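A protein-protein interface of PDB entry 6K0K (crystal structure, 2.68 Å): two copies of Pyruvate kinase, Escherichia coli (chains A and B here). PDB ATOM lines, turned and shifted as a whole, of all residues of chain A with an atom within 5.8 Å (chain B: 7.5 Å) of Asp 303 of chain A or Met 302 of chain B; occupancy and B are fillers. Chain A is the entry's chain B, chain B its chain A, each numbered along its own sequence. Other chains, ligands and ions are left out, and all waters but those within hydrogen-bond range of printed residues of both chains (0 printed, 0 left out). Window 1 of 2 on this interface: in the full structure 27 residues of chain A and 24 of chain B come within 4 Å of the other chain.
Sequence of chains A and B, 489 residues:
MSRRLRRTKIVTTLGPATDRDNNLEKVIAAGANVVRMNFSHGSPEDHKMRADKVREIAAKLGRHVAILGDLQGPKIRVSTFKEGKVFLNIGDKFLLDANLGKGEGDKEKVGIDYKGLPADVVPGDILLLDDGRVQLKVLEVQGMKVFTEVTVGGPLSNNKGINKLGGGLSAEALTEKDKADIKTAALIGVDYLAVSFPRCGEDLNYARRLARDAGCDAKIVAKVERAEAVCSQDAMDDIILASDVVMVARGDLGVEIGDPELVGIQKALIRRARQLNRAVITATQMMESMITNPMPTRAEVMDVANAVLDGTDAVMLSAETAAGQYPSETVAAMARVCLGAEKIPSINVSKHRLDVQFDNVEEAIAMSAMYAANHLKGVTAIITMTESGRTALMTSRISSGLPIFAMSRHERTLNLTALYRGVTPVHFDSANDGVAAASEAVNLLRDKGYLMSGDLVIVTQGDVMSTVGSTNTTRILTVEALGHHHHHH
Among the printed residues, merely in contact across the chains: Met 302 of chain A with Asp 303 of chain B (3.2 Å), Asp 303 of chain A with Met 302 of chain B (3.2 Å), Lys 267 of chain A with Leu 309 of chain B (3.4 Å), Gln 266 of chain A with Met 302 of chain B (3.6 Å), Val 263 of chain A with Ala 305 of chain B (3.6 Å), Ala 299 of chain A with Ala 299 of chain B (3.7 Å), Arg 250 of chain A with Arg 298 of chain B (3.7 Å), Val 263 of chain A with Met 302 of chain B (3.7 Å), Leu 262 of chain A with Arg 298 of chain B (3.8 Å), Met 302 of chain A with Val 263 of chain B (3.8 Å), Ala 305 of chain A with Val 263 of chain B (3.9 Å), Ala 299 of chain A with Glu 300 of chain B (3.9 Å), Asp 303 of chain A with Ala 299 of chain B (3.9 Å), Glu 300 of chain A with Ala 299 of chain B (3.9 Å) and Ala 299 of chain A with Asp 303 of chain B (3.99 Å).
Hydrophobic or aromatic side chains of chain B within 4 Å of the printed part of chain A: Val 263, Ala 299, Met 302, Ala 305 and Leu 309. Along chain B the printed residues that touch a printed residue of chain A span positions 263 to 309. Of the 19 printed residues of chain A, 11 touch a printed residue of chain B.
OD1 of Asn 306 of chain B sits at hydrogen-bond distance from NZ of Lys 267 of chain A. The side-chain amide oxygen (OD1) of Asn 306 of chain B lies close to the side-chain amide oxygen (OD1) of Asn 306 of chain A. The side-chain sulfur of Met 302 of chain B sits close to the guanidinium group of Arg 250 of chain A (3.7 Å).
The side-chain amino group of Lys 267 of chain A is in salt-bridge range of the side-chain carboxylate of Asp 310 of chain A, 3.2 Å away. The guanidinium group of Arg 250 of chain A lies within salt-bridge range of the side-chain carboxylate of Asp 303 of chain A. NE2 of Gln 266 of chain A is in hydrogen-bond range of OD2 of Asp 310 of chain A (3.0 Å). NH2 of Arg 250 of chain A sits at hydrogen-bond distance from SD of Met 286 of chain A. The backbone carbonyl oxygen (O) of Met 302 of chain B sits at hydrogen-bond distance from the side-chain amide nitrogen (ND2) of Asn 306 of chain B. O of Met 302 of chain A sits at hydrogen-bond distance from ND2 of Asn 306 of chain A (3.2 Å).
Of the printed residues of chain B, Lys 267 of chain A touches Asn 306 (3.0 Å) and Leu 309 (3.4 Å). Asp 303 of chain A touches just these residues of chain B: Ala 299 (3.9 Å) and Met 302 (3.2 Å). Ala 307 of chain A touches none of the printed residues of chain B. Asp 310 of chain A touches none of the printed residues of chain B. Of the printed residues of chain A, Val 263 of chain B touches Met 302 and Ala 305. Of the printed residues of chain A, Glu 300 of chain B touches Ala 299 (3.9 Å). Printed residues of chain A within 4 Å of Ala 305 of chain B: Val 263 (3.6 Å). The nearest residue of chain B that does not touch Asp 303 of chain A is Arg 298 of chain B (4.9 Å). The nearest printed residue of chain B that does not touch Leu 262 of chain A is Met 302 of chain B (5.1 Å).
Val 263 of chain A touches Met 302 of chain B, and with the chains exchanged Met 302 of chain A touches Val 263 of chain B. Val 263 of chain A touches Ala 305 of chain B, and with the chains exchanged Ala 305 of chain A touches Val 263 of chain B. Ala 299 of chain B touches its own counterpart, Ala 299 of chain A. Met 302 of chain A touches Asp 303 of chain B, and with the chains exchanged Asp 303 of chain A touches Met 302 of chain B.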
ATOM      1  N   ARG A 250      -0.013  18.937  12.558  1.00  0.00           N
ATOM      2  CA  ARG A 250      -0.424  17.861  11.645  1.00  0.00           C
ATOM      3  C   ARG A 250       0.742  17.227  10.893  1.00  0.00           C
ATOM      4  O   ARG A 250       0.652  16.052  10.517  1.00  0.00           O
ATOM      5  CB  ARG A 250      -1.445  18.388  10.649  1.00  0.00           C
ATOM      6  CG  ARG A 250      -2.589  19.058  11.327  1.00  0.00           C
ATOM      7  CD  ARG A 250      -3.717  19.238  10.370  1.00  0.00           C
ATOM      8  NE  ARG A 250      -3.482  20.296   9.410  1.00  0.00           N
ATOM      9  CZ  ARG A 250      -4.424  20.739   8.591  1.00  0.00           C
ATOM     10  NH1 ARG A 250      -5.633  20.202   8.657  1.00  0.00           N
ATOM     11  NH2 ARG A 250      -4.170  21.716   7.726  1.00  0.00           N
ATOM     12  N   LEU A 262      -5.780  11.322  11.091  1.00  0.00           N
ATOM     13  CA  LEU A 262      -5.451  12.663  11.542  1.00  0.00           C
ATOM     14  C   LEU A 262      -6.668  13.573  11.560  1.00  0.00           C
ATOM     15  O   LEU A 262      -6.753  14.472  12.395  1.00  0.00           O
ATOM     16  CB  LEU A 262      -4.360  13.236  10.650  1.00  0.00           C
ATOM     17  CG  LEU A 262      -3.847  14.608  11.042  1.00  0.00           C
ATOM     18  CD1 LEU A 262      -3.330  14.522  12.447  1.00  0.00           C
ATOM     19  CD2 LEU A 262      -2.761  15.005  10.062  1.00  0.00           C
ATOM     20  N   VAL A 263      -7.616  13.351  10.662  1.00  0.00           N
ATOM     21  CA  VAL A 263      -8.809  14.189  10.597  1.00  0.00           C
ATOM     22  C   VAL A 263      -9.597  14.087  11.895  1.00  0.00           C
ATOM     23  O   VAL A 263      -9.891  15.093  12.561  1.00  0.00           O
ATOM     24  CB  VAL A 263      -9.669  13.775   9.390  1.00  0.00           C
ATOM     25  CG1 VAL A 263     -10.778  14.764   9.175  1.00  0.00           C
ATOM     26  CG2 VAL A 263      -8.785  13.595   8.111  1.00  0.00           C
ATOM     27  N   GLN A 266      -7.659  15.558  14.842  1.00  0.00           N
ATOM     28  CA  GLN A 266      -7.730  17.014  14.904  1.00  0.00           C
ATOM     29  C   GLN A 266      -9.063  17.439  15.477  1.00  0.00           C
ATOM     30  O   GLN A 266      -9.128  18.334  16.330  1.00  0.00           O
ATOM     31  CB  GLN A 266      -7.519  17.629  13.512  1.00  0.00           C
ATOM     32  CG  GLN A 266      -7.978  19.088  13.344  1.00  0.00           C
ATOM     33  CD  GLN A 266      -7.813  19.595  11.906  1.00  0.00           C
ATOM     34  OE1 GLN A 266      -6.810  19.312  11.267  1.00  0.00           O
ATOM     35  NE2 GLN A 266      -8.803  20.331  11.395  1.00  0.00           N
ATOM     36  N   LYS A 267     -10.139  16.787  15.031  1.00  0.00           N
ATOM     37  CA  LYS A 267     -11.470  17.205  15.442  1.00  0.00           C
ATOM     38  C   LYS A 267     -11.671  16.966  16.930  1.00  0.00           C
ATOM     39  O   LYS A 267     -12.133  17.858  17.663  1.00  0.00           O
ATOM     40  CB  LYS A 267     -12.511  16.467  14.602  1.00  0.00           C
ATOM     41  CG  LYS A 267     -12.587  17.010  13.180  1.00  0.00           C
ATOM     42  CD  LYS A 267     -13.111  15.985  12.181  1.00  0.00           C
ATOM     43  CE  LYS A 267     -13.181  16.580  10.783  1.00  0.00           C
ATOM     44  NZ  LYS A 267     -14.518  17.122  10.447  1.00  0.00           N
ATOM     45  N   GLN A 285       1.406  24.747   7.390  1.00  0.00           N
ATOM     46  CA  GLN A 285       1.294  24.552   5.945  1.00  0.00           C
ATOM     47  C   GLN A 285      -0.163  24.421   5.512  1.00  0.00           C
ATOM     48  O   GLN A 285      -0.530  23.528   4.743  1.00  0.00           O
ATOM     49  CB  GLN A 285       2.111  23.335   5.495  1.00  0.00           C
ATOM     50  CG  GLN A 285       3.579  23.361   5.955  1.00  0.00           C
ATOM     51  CD  GLN A 285       4.395  24.435   5.244  1.00  0.00           C
ATOM     52  OE1 GLN A 285       5.169  25.166   5.872  1.00  0.00           O
ATOM     53  NE2 GLN A 285       4.228  24.529   3.924  1.00  0.00           N
ATOM     54  N   MET A 286      -1.001  25.334   6.008  1.00  0.00           N
ATOM     55  CA  MET A 286      -2.416  25.289   5.659  1.00  0.00           C
ATOM     56  C   MET A 286      -2.656  25.682   4.207  1.00  0.00           C
ATOM     57  O   MET A 286      -3.659  25.269   3.617  1.00  0.00           O
ATOM     58  CB  MET A 286      -3.217  26.200   6.582  1.00  0.00           C
ATOM     59  CG  MET A 286      -2.973  25.981   8.072  1.00  0.00           C
ATOM     60  SD  MET A 286      -4.141  24.827   8.788  1.00  0.00           S
ATOM     61  CE  MET A 286      -5.651  25.729   8.446  1.00  0.00           C
ATOM     62  N   ARG A 298      -7.844  24.465  -4.122  1.00  0.00           N
ATOM     63  CA  ARG A 298      -9.196  24.325  -3.584  1.00  0.00           C
ATOM     64  C   ARG A 298      -9.210  23.419  -2.352  1.00  0.00           C
ATOM     65  O   ARG A 298      -9.948  23.677  -1.391  1.00  0.00           O
ATOM     66  CB  ARG A 298     -10.143  23.800  -4.675  1.00  0.00           C
ATOM     67  CG  ARG A 298     -11.582  23.523  -4.213  1.00  0.00           C
ATOM     68  CD  ARG A 298     -12.517  23.255  -5.385  1.00  0.00           C
ATOM     69  NE  ARG A 298     -12.575  24.400  -6.295  1.00  0.00           N
ATOM     70  CZ  ARG A 298     -12.085  24.406  -7.537  1.00  0.00           C
ATOM     71  NH1 ARG A 298     -11.505  23.308  -8.039  1.00  0.00           N
ATOM     72  NH2 ARG A 298     -12.178  25.515  -8.284  1.00  0.00           N
ATOM     73  N   ALA A 299      -8.400  22.355  -2.362  1.00  0.00           N
ATOM     74  CA  ALA A 299      -8.305  21.491  -1.192  1.00  0.00           C
ATOM     75  C   ALA A 299      -7.735  22.241   0.000  1.00  0.00           C
ATOM     76  O   ALA A 299      -8.103  21.955   1.143  1.00  0.00           O
ATOM     77  CB  ALA A 299      -7.455  20.242  -1.485  1.00  0.00           C
ATOM     78  N   GLU A 300      -6.839  23.195  -0.235  1.00  0.00           N
ATOM     79  CA  GLU A 300      -6.340  23.983   0.886  1.00  0.00           C
ATOM     80  C   GLU A 300      -7.459  24.834   1.480  1.00  0.00           C
ATOM     81  O   GLU A 300      -7.615  24.901   2.707  1.00  0.00           O
ATOM     82  CB  GLU A 300      -5.145  24.837   0.441  1.00  0.00           C
ATOM     83  CG  GLU A 300      -3.803  24.076   0.452  1.00  0.00           C
ATOM     84  CD  GLU A 300      -2.763  24.654  -0.501  1.00  0.00           C
ATOM     85  OE1 GLU A 300      -3.043  25.685  -1.151  1.00  0.00           O
ATOM     86  OE2 GLU A 300      -1.667  24.070  -0.609  1.00  0.00           O
ATOM     87  N   VAL A 301      -8.268  25.455   0.620  1.00  0.00           N
ATOM     88  CA  VAL A 301      -9.424  26.214   1.078  1.00  0.00           C
ATOM     89  C   VAL A 301     -10.375  25.316   1.856  1.00  0.00           C
ATOM     90  O   VAL A 301     -10.948  25.719   2.877  1.00  0.00           O
ATOM     91  CB  VAL A 301     -10.117  26.870  -0.132  1.00  0.00           C
ATOM     92  CG1 VAL A 301     -11.422  27.581   0.278  1.00  0.00           C
ATOM     93  CG2 VAL A 301      -9.173  27.820  -0.804  1.00  0.00           C
ATOM     94  N   MET A 302     -10.557  24.087   1.383  1.00  0.00           N
ATOM     95  CA  MET A 302     -11.444  23.152   2.057  1.00  0.00           C
ATOM     96  C   MET A 302     -10.890  22.785   3.422  1.00  0.00           C
ATOM     97  O   MET A 302     -11.609  22.799   4.429  1.00  0.00           O
ATOM     98  CB  MET A 302     -11.649  21.907   1.189  1.00  0.00           C
ATOM     99  CG  MET A 302     -12.398  22.158  -0.113  1.00  0.00           C
ATOM    100  SD  MET A 302     -14.210  22.251   0.060  1.00  0.00           S
ATOM    101  CE  MET A 302     -14.599  20.605   0.672  1.00  0.00           C
ATOM    102  N   ASP A 303      -9.599  22.480   3.474  1.00  0.00           N
ATOM    103  CA  ASP A 303      -8.936  22.180   4.733  1.00  0.00           C
ATOM    104  C   ASP A 303      -9.125  23.319   5.737  1.00  0.00           C
ATOM    105  O   ASP A 303      -9.606  23.116   6.863  1.00  0.00           O
ATOM    106  CB  ASP A 303      -7.456  21.932   4.442  1.00  0.00           C
ATOM    107  CG  ASP A 303      -6.739  21.308   5.598  1.00  0.00           C
ATOM    108  OD1 ASP A 303      -7.428  20.941   6.579  1.00  0.00           O
ATOM    109  OD2 ASP A 303      -5.497  21.180   5.524  1.00  0.00           O
ATOM    110  N   VAL A 304      -8.749  24.531   5.321  1.00  0.00           N
ATOM    111  CA  VAL A 304      -8.807  25.709   6.179  1.00  0.00           C
ATOM    112  C   VAL A 304     -10.221  25.928   6.703  1.00  0.00           C
ATOM    113  O   VAL A 304     -10.441  26.105   7.917  1.00  0.00           O
ATOM    114  CB  VAL A 304      -8.298  26.939   5.403  1.00  0.00           C
ATOM    115  CG1 VAL A 304      -8.533  28.211   6.176  1.00  0.00           C
ATOM    116  CG2 VAL A 304      -6.850  26.767   5.063  1.00  0.00           C
ATOM    117  N   ALA A 305     -11.203  25.936   5.790  1.00  0.00           N
ATOM    118  CA  ALA A 305     -12.571  26.226   6.196  1.00  0.00           C
ATOM    119  C   ALA A 305     -13.136  25.123   7.078  1.00  0.00           C
ATOM    120  O   ALA A 305     -13.916  25.410   7.993  1.00  0.00           O
ATOM    121  CB  ALA A 305     -13.455  26.432   4.971  1.00  0.00           C
ATOM    122  N   ASN A 306     -12.747  23.866   6.852  1.00  0.00           N
ATOM    123  CA  ASN A 306     -13.219  22.830   7.762  1.00  0.00           C
ATOM    124  C   ASN A 306     -12.565  22.930   9.135  1.00  0.00           C
ATOM    125  O   ASN A 306     -13.186  22.532  10.116  1.00  0.00           O
ATOM    126  CB  ASN A 306     -13.031  21.435   7.160  1.00  0.00           C
ATOM    127  CG  ASN A 306     -14.250  20.978   6.374  1.00  0.00           C
ATOM    128  OD1 ASN A 306     -15.335  20.755   6.952  1.00  0.00           O
ATOM    129  ND2 ASN A 306     -14.097  20.865   5.052  1.00  0.00           N
ATOM    130  N   ALA A 307     -11.337  23.462   9.251  1.00  0.00           N
ATOM    131  CA  ALA A 307     -10.807  23.690  10.606  1.00  0.00           C
ATOM    132  C   ALA A 307     -11.576  24.812  11.307  1.00  0.00           C
ATOM    133  O   ALA A 307     -11.816  24.759  12.520  1.00  0.00           O
ATOM    134  CB  ALA A 307      -9.311  24.013  10.577  1.00  0.00           C
ATOM    135  N   VAL A 308     -11.976  25.837  10.550  1.00  0.00           N
ATOM    136  CA  VAL A 308     -12.891  26.824  11.103  1.00  0.00           C
ATOM    137  C   VAL A 308     -14.150  26.140  11.623  1.00  0.00           C
ATOM    138  O   VAL A 308     -14.532  26.305  12.787  1.00  0.00           O
ATOM    139  CB  VAL A 308     -13.226  27.892  10.053  1.00  0.00           C
ATOM    140  CG1 VAL A 308     -14.256  28.899  10.622  1.00  0.00           C
ATOM    141  CG2 VAL A 308     -11.962  28.572   9.573  1.00  0.00           C
ATOM    142  N   ASP A 310     -14.604  23.109  12.422  1.00  0.00           N
ATOM    143  CA  ASP A 310     -14.211  22.247  13.528  1.00  0.00           C
ATOM    144  C   ASP A 310     -14.179  23.017  14.833  1.00  0.00           C
ATOM    145  O   ASP A 310     -14.254  22.402  15.904  1.00  0.00           O
ATOM    146  CB  ASP A 310     -12.832  21.630  13.274  1.00  0.00           C
ATOM    147  CG  ASP A 310     -12.859  20.452  12.291  1.00  0.00           C
ATOM    148  OD1 ASP A 310     -13.931  19.852  12.106  1.00  0.00           O
ATOM    149  OD2 ASP A 310     -11.796  20.121  11.703  1.00  0.00           O
ATOM    150  N   VAL B 263     -17.854  25.693   0.295  1.00  0.00           N
ATOM    151  CA  VAL B 263     -17.877  24.671   1.346  1.00  0.00           C
ATOM    152  C   VAL B 263     -19.281  24.534   1.928  1.00  0.00           C
ATOM    153  O   VAL B 263     -19.818  23.422   2.086  1.00  0.00           O
ATOM    154  CB  VAL B 263     -16.861  24.991   2.459  1.00  0.00           C
ATOM    155  CG1 VAL B 263     -16.751  23.779   3.389  1.00  0.00           C
ATOM    156  CG2 VAL B 263     -15.511  25.343   1.892  1.00  0.00           C
ATOM    157  N   THR B 297      -1.526  15.134  -1.178  1.00  0.00           N
ATOM    158  CA  THR B 297      -1.431  16.268  -0.274  1.00  0.00           C
ATOM    159  C   THR B 297      -2.266  16.033   0.989  1.00  0.00           C
ATOM    160  O   THR B 297      -3.323  15.392   0.953  1.00  0.00           O
ATOM    161  CB  THR B 297      -1.904  17.501  -1.042  1.00  0.00           C
ATOM    162  OG1 THR B 297      -0.798  18.050  -1.766  1.00  0.00           O
ATOM    163  CG2 THR B 297      -2.522  18.553  -0.177  1.00  0.00           C
ATOM    164  N   ARG B 298      -1.773  16.541   2.124  1.00  0.00           N
ATOM    165  CA  ARG B 298      -2.551  16.466   3.360  1.00  0.00           C
ATOM    166  C   ARG B 298      -3.893  17.172   3.203  1.00  0.00           C
ATOM    167  O   ARG B 298      -4.936  16.640   3.611  1.00  0.00           O
ATOM    168  CB  ARG B 298      -1.760  17.053   4.533  1.00  0.00           C
ATOM    169  CG  ARG B 298      -2.346  16.709   5.906  1.00  0.00           C
ATOM    170  CD  ARG B 298      -1.288  16.699   7.035  1.00  0.00           C
ATOM    171  NE  ARG B 298      -0.325  15.582   6.988  1.00  0.00           N
ATOM    172  CZ  ARG B 298       0.991  15.716   6.781  1.00  0.00           C
ATOM    173  NH1 ARG B 298       1.525  16.926   6.598  1.00  0.00           N
ATOM    174  NH2 ARG B 298       1.782  14.640   6.759  1.00  0.00           N
ATOM    175  N   ALA B 299      -3.885  18.360   2.587  1.00  0.00           N
ATOM    176  CA  ALA B 299      -5.128  19.076   2.293  1.00  0.00           C
ATOM    177  C   ALA B 299      -6.088  18.232   1.463  1.00  0.00           C
ATOM    178  O   ALA B 299      -7.298  18.254   1.701  1.00  0.00           O
ATOM    179  CB  ALA B 299      -4.830  20.393   1.568  1.00  0.00           C
ATOM    180  N   GLU B 300      -5.568  17.494   0.473  1.00  0.00           N
ATOM    181  CA  GLU B 300      -6.409  16.625  -0.350  1.00  0.00           C
ATOM    182  C   GLU B 300      -7.032  15.504   0.476  1.00  0.00           C
ATOM    183  O   GLU B 300      -8.206  15.159   0.289  1.00  0.00           O
ATOM    184  CB  GLU B 300      -5.583  16.056  -1.507  1.00  0.00           C
ATOM    185  CG  GLU B 300      -5.193  17.102  -2.556  1.00  0.00           C
ATOM    186  CD  GLU B 300      -4.155  16.591  -3.546  1.00  0.00           C
ATOM    187  OE1 GLU B 300      -3.700  15.431  -3.374  1.00  0.00           O
ATOM    188  OE2 GLU B 300      -3.792  17.347  -4.484  1.00  0.00           O
ATOM    189  N   VAL B 301      -6.257  14.928   1.394  1.00  0.00           N
ATOM    190  CA  VAL B 301      -6.786  13.950   2.341  1.00  0.00           C
ATOM    191  C   VAL B 301      -7.941  14.551   3.139  1.00  0.00           C
ATOM    192  O   VAL B 301      -9.014  13.945   3.262  1.00  0.00           O
ATOM    193  CB  VAL B 301      -5.667  13.455   3.278  1.00  0.00           C
ATOM    194  CG1 VAL B 301      -6.223  12.513   4.345  1.00  0.00           C
ATOM    195  CG2 VAL B 301      -4.565  12.801   2.500  1.00  0.00           C
ATOM    196  N   MET B 302      -7.714  15.731   3.729  1.00  0.00           N
ATOM    197  CA  MET B 302      -8.728  16.372   4.566  1.00  0.00           C
ATOM    198  C   MET B 302      -9.964  16.721   3.755  1.00  0.00           C
ATOM    199  O   MET B 302     -11.091  16.654   4.259  1.00  0.00           O
ATOM    200  CB  MET B 302      -8.168  17.646   5.216  1.00  0.00           C
ATOM    201  CG  MET B 302      -6.970  17.459   6.153  1.00  0.00           C
ATOM    202  SD  MET B 302      -7.438  17.051   7.852  1.00  0.00           S
ATOM    203  CE  MET B 302      -8.513  18.446   8.219  1.00  0.00           C
ATOM    204  N   ASP B 303      -9.763  17.106   2.495  1.00  0.00           N
ATOM    205  CA  ASP B 303     -10.873  17.351   1.588  1.00  0.00           C
ATOM    206  C   ASP B 303     -11.721  16.094   1.445  1.00  0.00           C
ATOM    207  O   ASP B 303     -12.915  16.091   1.779  1.00  0.00           O
ATOM    208  CB  ASP B 303     -10.335  17.814   0.233  1.00  0.00           C
ATOM    209  CG  ASP B 303     -11.434  18.304  -0.708  1.00  0.00           C
ATOM    210  OD1 ASP B 303     -12.621  18.326  -0.299  1.00  0.00           O
ATOM    211  OD2 ASP B 303     -11.103  18.676  -1.867  1.00  0.00           O
ATOM    212  N   VAL B 304     -11.110  15.011   0.962  1.00  0.00           N
ATOM    213  CA  VAL B 304     -11.844  13.763   0.772  1.00  0.00           C
ATOM    214  C   VAL B 304     -12.539  13.345   2.064  1.00  0.00           C
ATOM    215  O   VAL B 304     -13.721  12.973   2.062  1.00  0.00           O
ATOM    216  CB  VAL B 304     -10.905  12.662   0.267  1.00  0.00           C
ATOM    217  CG1 VAL B 304     -11.594  11.306   0.366  1.00  0.00           C
ATOM    218  CG2 VAL B 304     -10.435  12.962  -1.151  1.00  0.00           C
ATOM    219  N   ALA B 305     -11.814  13.405   3.184  1.00  0.00           N
ATOM    220  CA  ALA B 305     -12.353  12.948   4.459  1.00  0.00           C
ATOM    221  C   ALA B 305     -13.543  13.794   4.897  1.00  0.00           C
ATOM    222  O   ALA B 305     -14.524  13.272   5.450  1.00  0.00           O
ATOM    223  CB  ALA B 305     -11.254  12.973   5.524  1.00  0.00           C
ATOM    224  N   ASN B 306     -13.490  15.105   4.652  1.00  0.00           N
ATOM    225  CA  ASN B 306     -14.645  15.906   5.013  1.00  0.00           C
ATOM    226  C   ASN B 306     -15.788  15.732   4.020  1.00  0.00           C
ATOM    227  O   ASN B 306     -16.953  15.929   4.384  1.00  0.00           O
ATOM    228  CB  ASN B 306     -14.249  17.382   5.165  1.00  0.00           C
ATOM    229  CG  ASN B 306     -13.559  17.669   6.494  1.00  0.00           C
ATOM    230  OD1 ASN B 306     -14.206  17.754   7.535  1.00  0.00           O
ATOM    231  ND2 ASN B 306     -12.243  17.810   6.459  1.00  0.00           N
ATOM    232  N   ALA B 307     -15.500  15.358   2.775  1.00  0.00           N
ATOM    233  CA  ALA B 307     -16.612  15.003   1.897  1.00  0.00           C
ATOM    234  C   ALA B 307     -17.288  13.754   2.418  1.00  0.00           C
ATOM    235  O   ALA B 307     -18.515  13.695   2.505  1.00  0.00           O
ATOM    236  CB  ALA B 307     -16.151  14.805   0.447  1.00  0.00           C
ATOM    237  N   VAL B 308     -16.494  12.773   2.836  1.00  0.00           N
ATOM    238  CA  VAL B 308     -17.051  11.581   3.455  1.00  0.00           C
ATOM    239  C   VAL B 308     -17.895  11.965   4.665  1.00  0.00           C
ATOM    240  O   VAL B 308     -19.055  11.562   4.786  1.00  0.00           O
ATOM    241  CB  VAL B 308     -15.926  10.598   3.823  1.00  0.00           C
ATOM    242  CG1 VAL B 308     -16.472   9.384   4.519  1.00  0.00           C
ATOM    243  CG2 VAL B 308     -15.172  10.178   2.585  1.00  0.00           C
ATOM    244  N   LEU B 309     -17.345  12.781   5.562  1.00  0.00           N
ATOM    245  CA  LEU B 309     -18.107  13.105   6.761  1.00  0.00           C
ATOM    246  C   LEU B 309     -19.326  13.949   6.450  1.00  0.00           C
ATOM    247  O   LEU B 309     -20.237  14.002   7.282  1.00  0.00           O
ATOM    248  CB  LEU B 309     -17.255  13.831   7.806  1.00  0.00           C
ATOM    249  CG  LEU B 309     -16.041  13.110   8.395  1.00  0.00           C
ATOM    250  CD1 LEU B 309     -15.391  13.956   9.450  1.00  0.00           C
ATOM    251  CD2 LEU B 309     -16.412  11.754   8.950  1.00  0.00           C
ATOM    252  N   VAL B 337      -8.251   6.738   2.520  1.00  0.00           N
ATOM    253  CA  VAL B 337      -8.777   7.940   3.160  1.00  0.00           C
ATOM    254  C   VAL B 337     -10.215   7.704   3.592  1.00  0.00           C
ATOM    255  O   VAL B 337     -10.606   8.029   4.718  1.00  0.00           O
ATOM    256  CB  VAL B 337      -8.672   9.176   2.245  1.00  0.00           C
ATOM    257  CG1 VAL B 337      -9.366  10.368   2.930  1.00  0.00           C
ATOM    258  CG2 VAL B 337      -7.215   9.533   1.949  1.00  0.00           C
ATOM    259  N   ALA B 341     -11.771   7.988   7.360  1.00  0.00           N
ATOM    260  CA  ALA B 341     -12.809   8.939   7.735  1.00  0.00           C
ATOM    261  C   ALA B 341     -14.079   8.247   8.229  1.00  0.00           C
ATOM    262  O   ALA B 341     -14.800   8.798   9.064  1.00  0.00           O
ATOM    263  CB  ALA B 341     -13.106   9.849   6.557  1.00  0.00           C
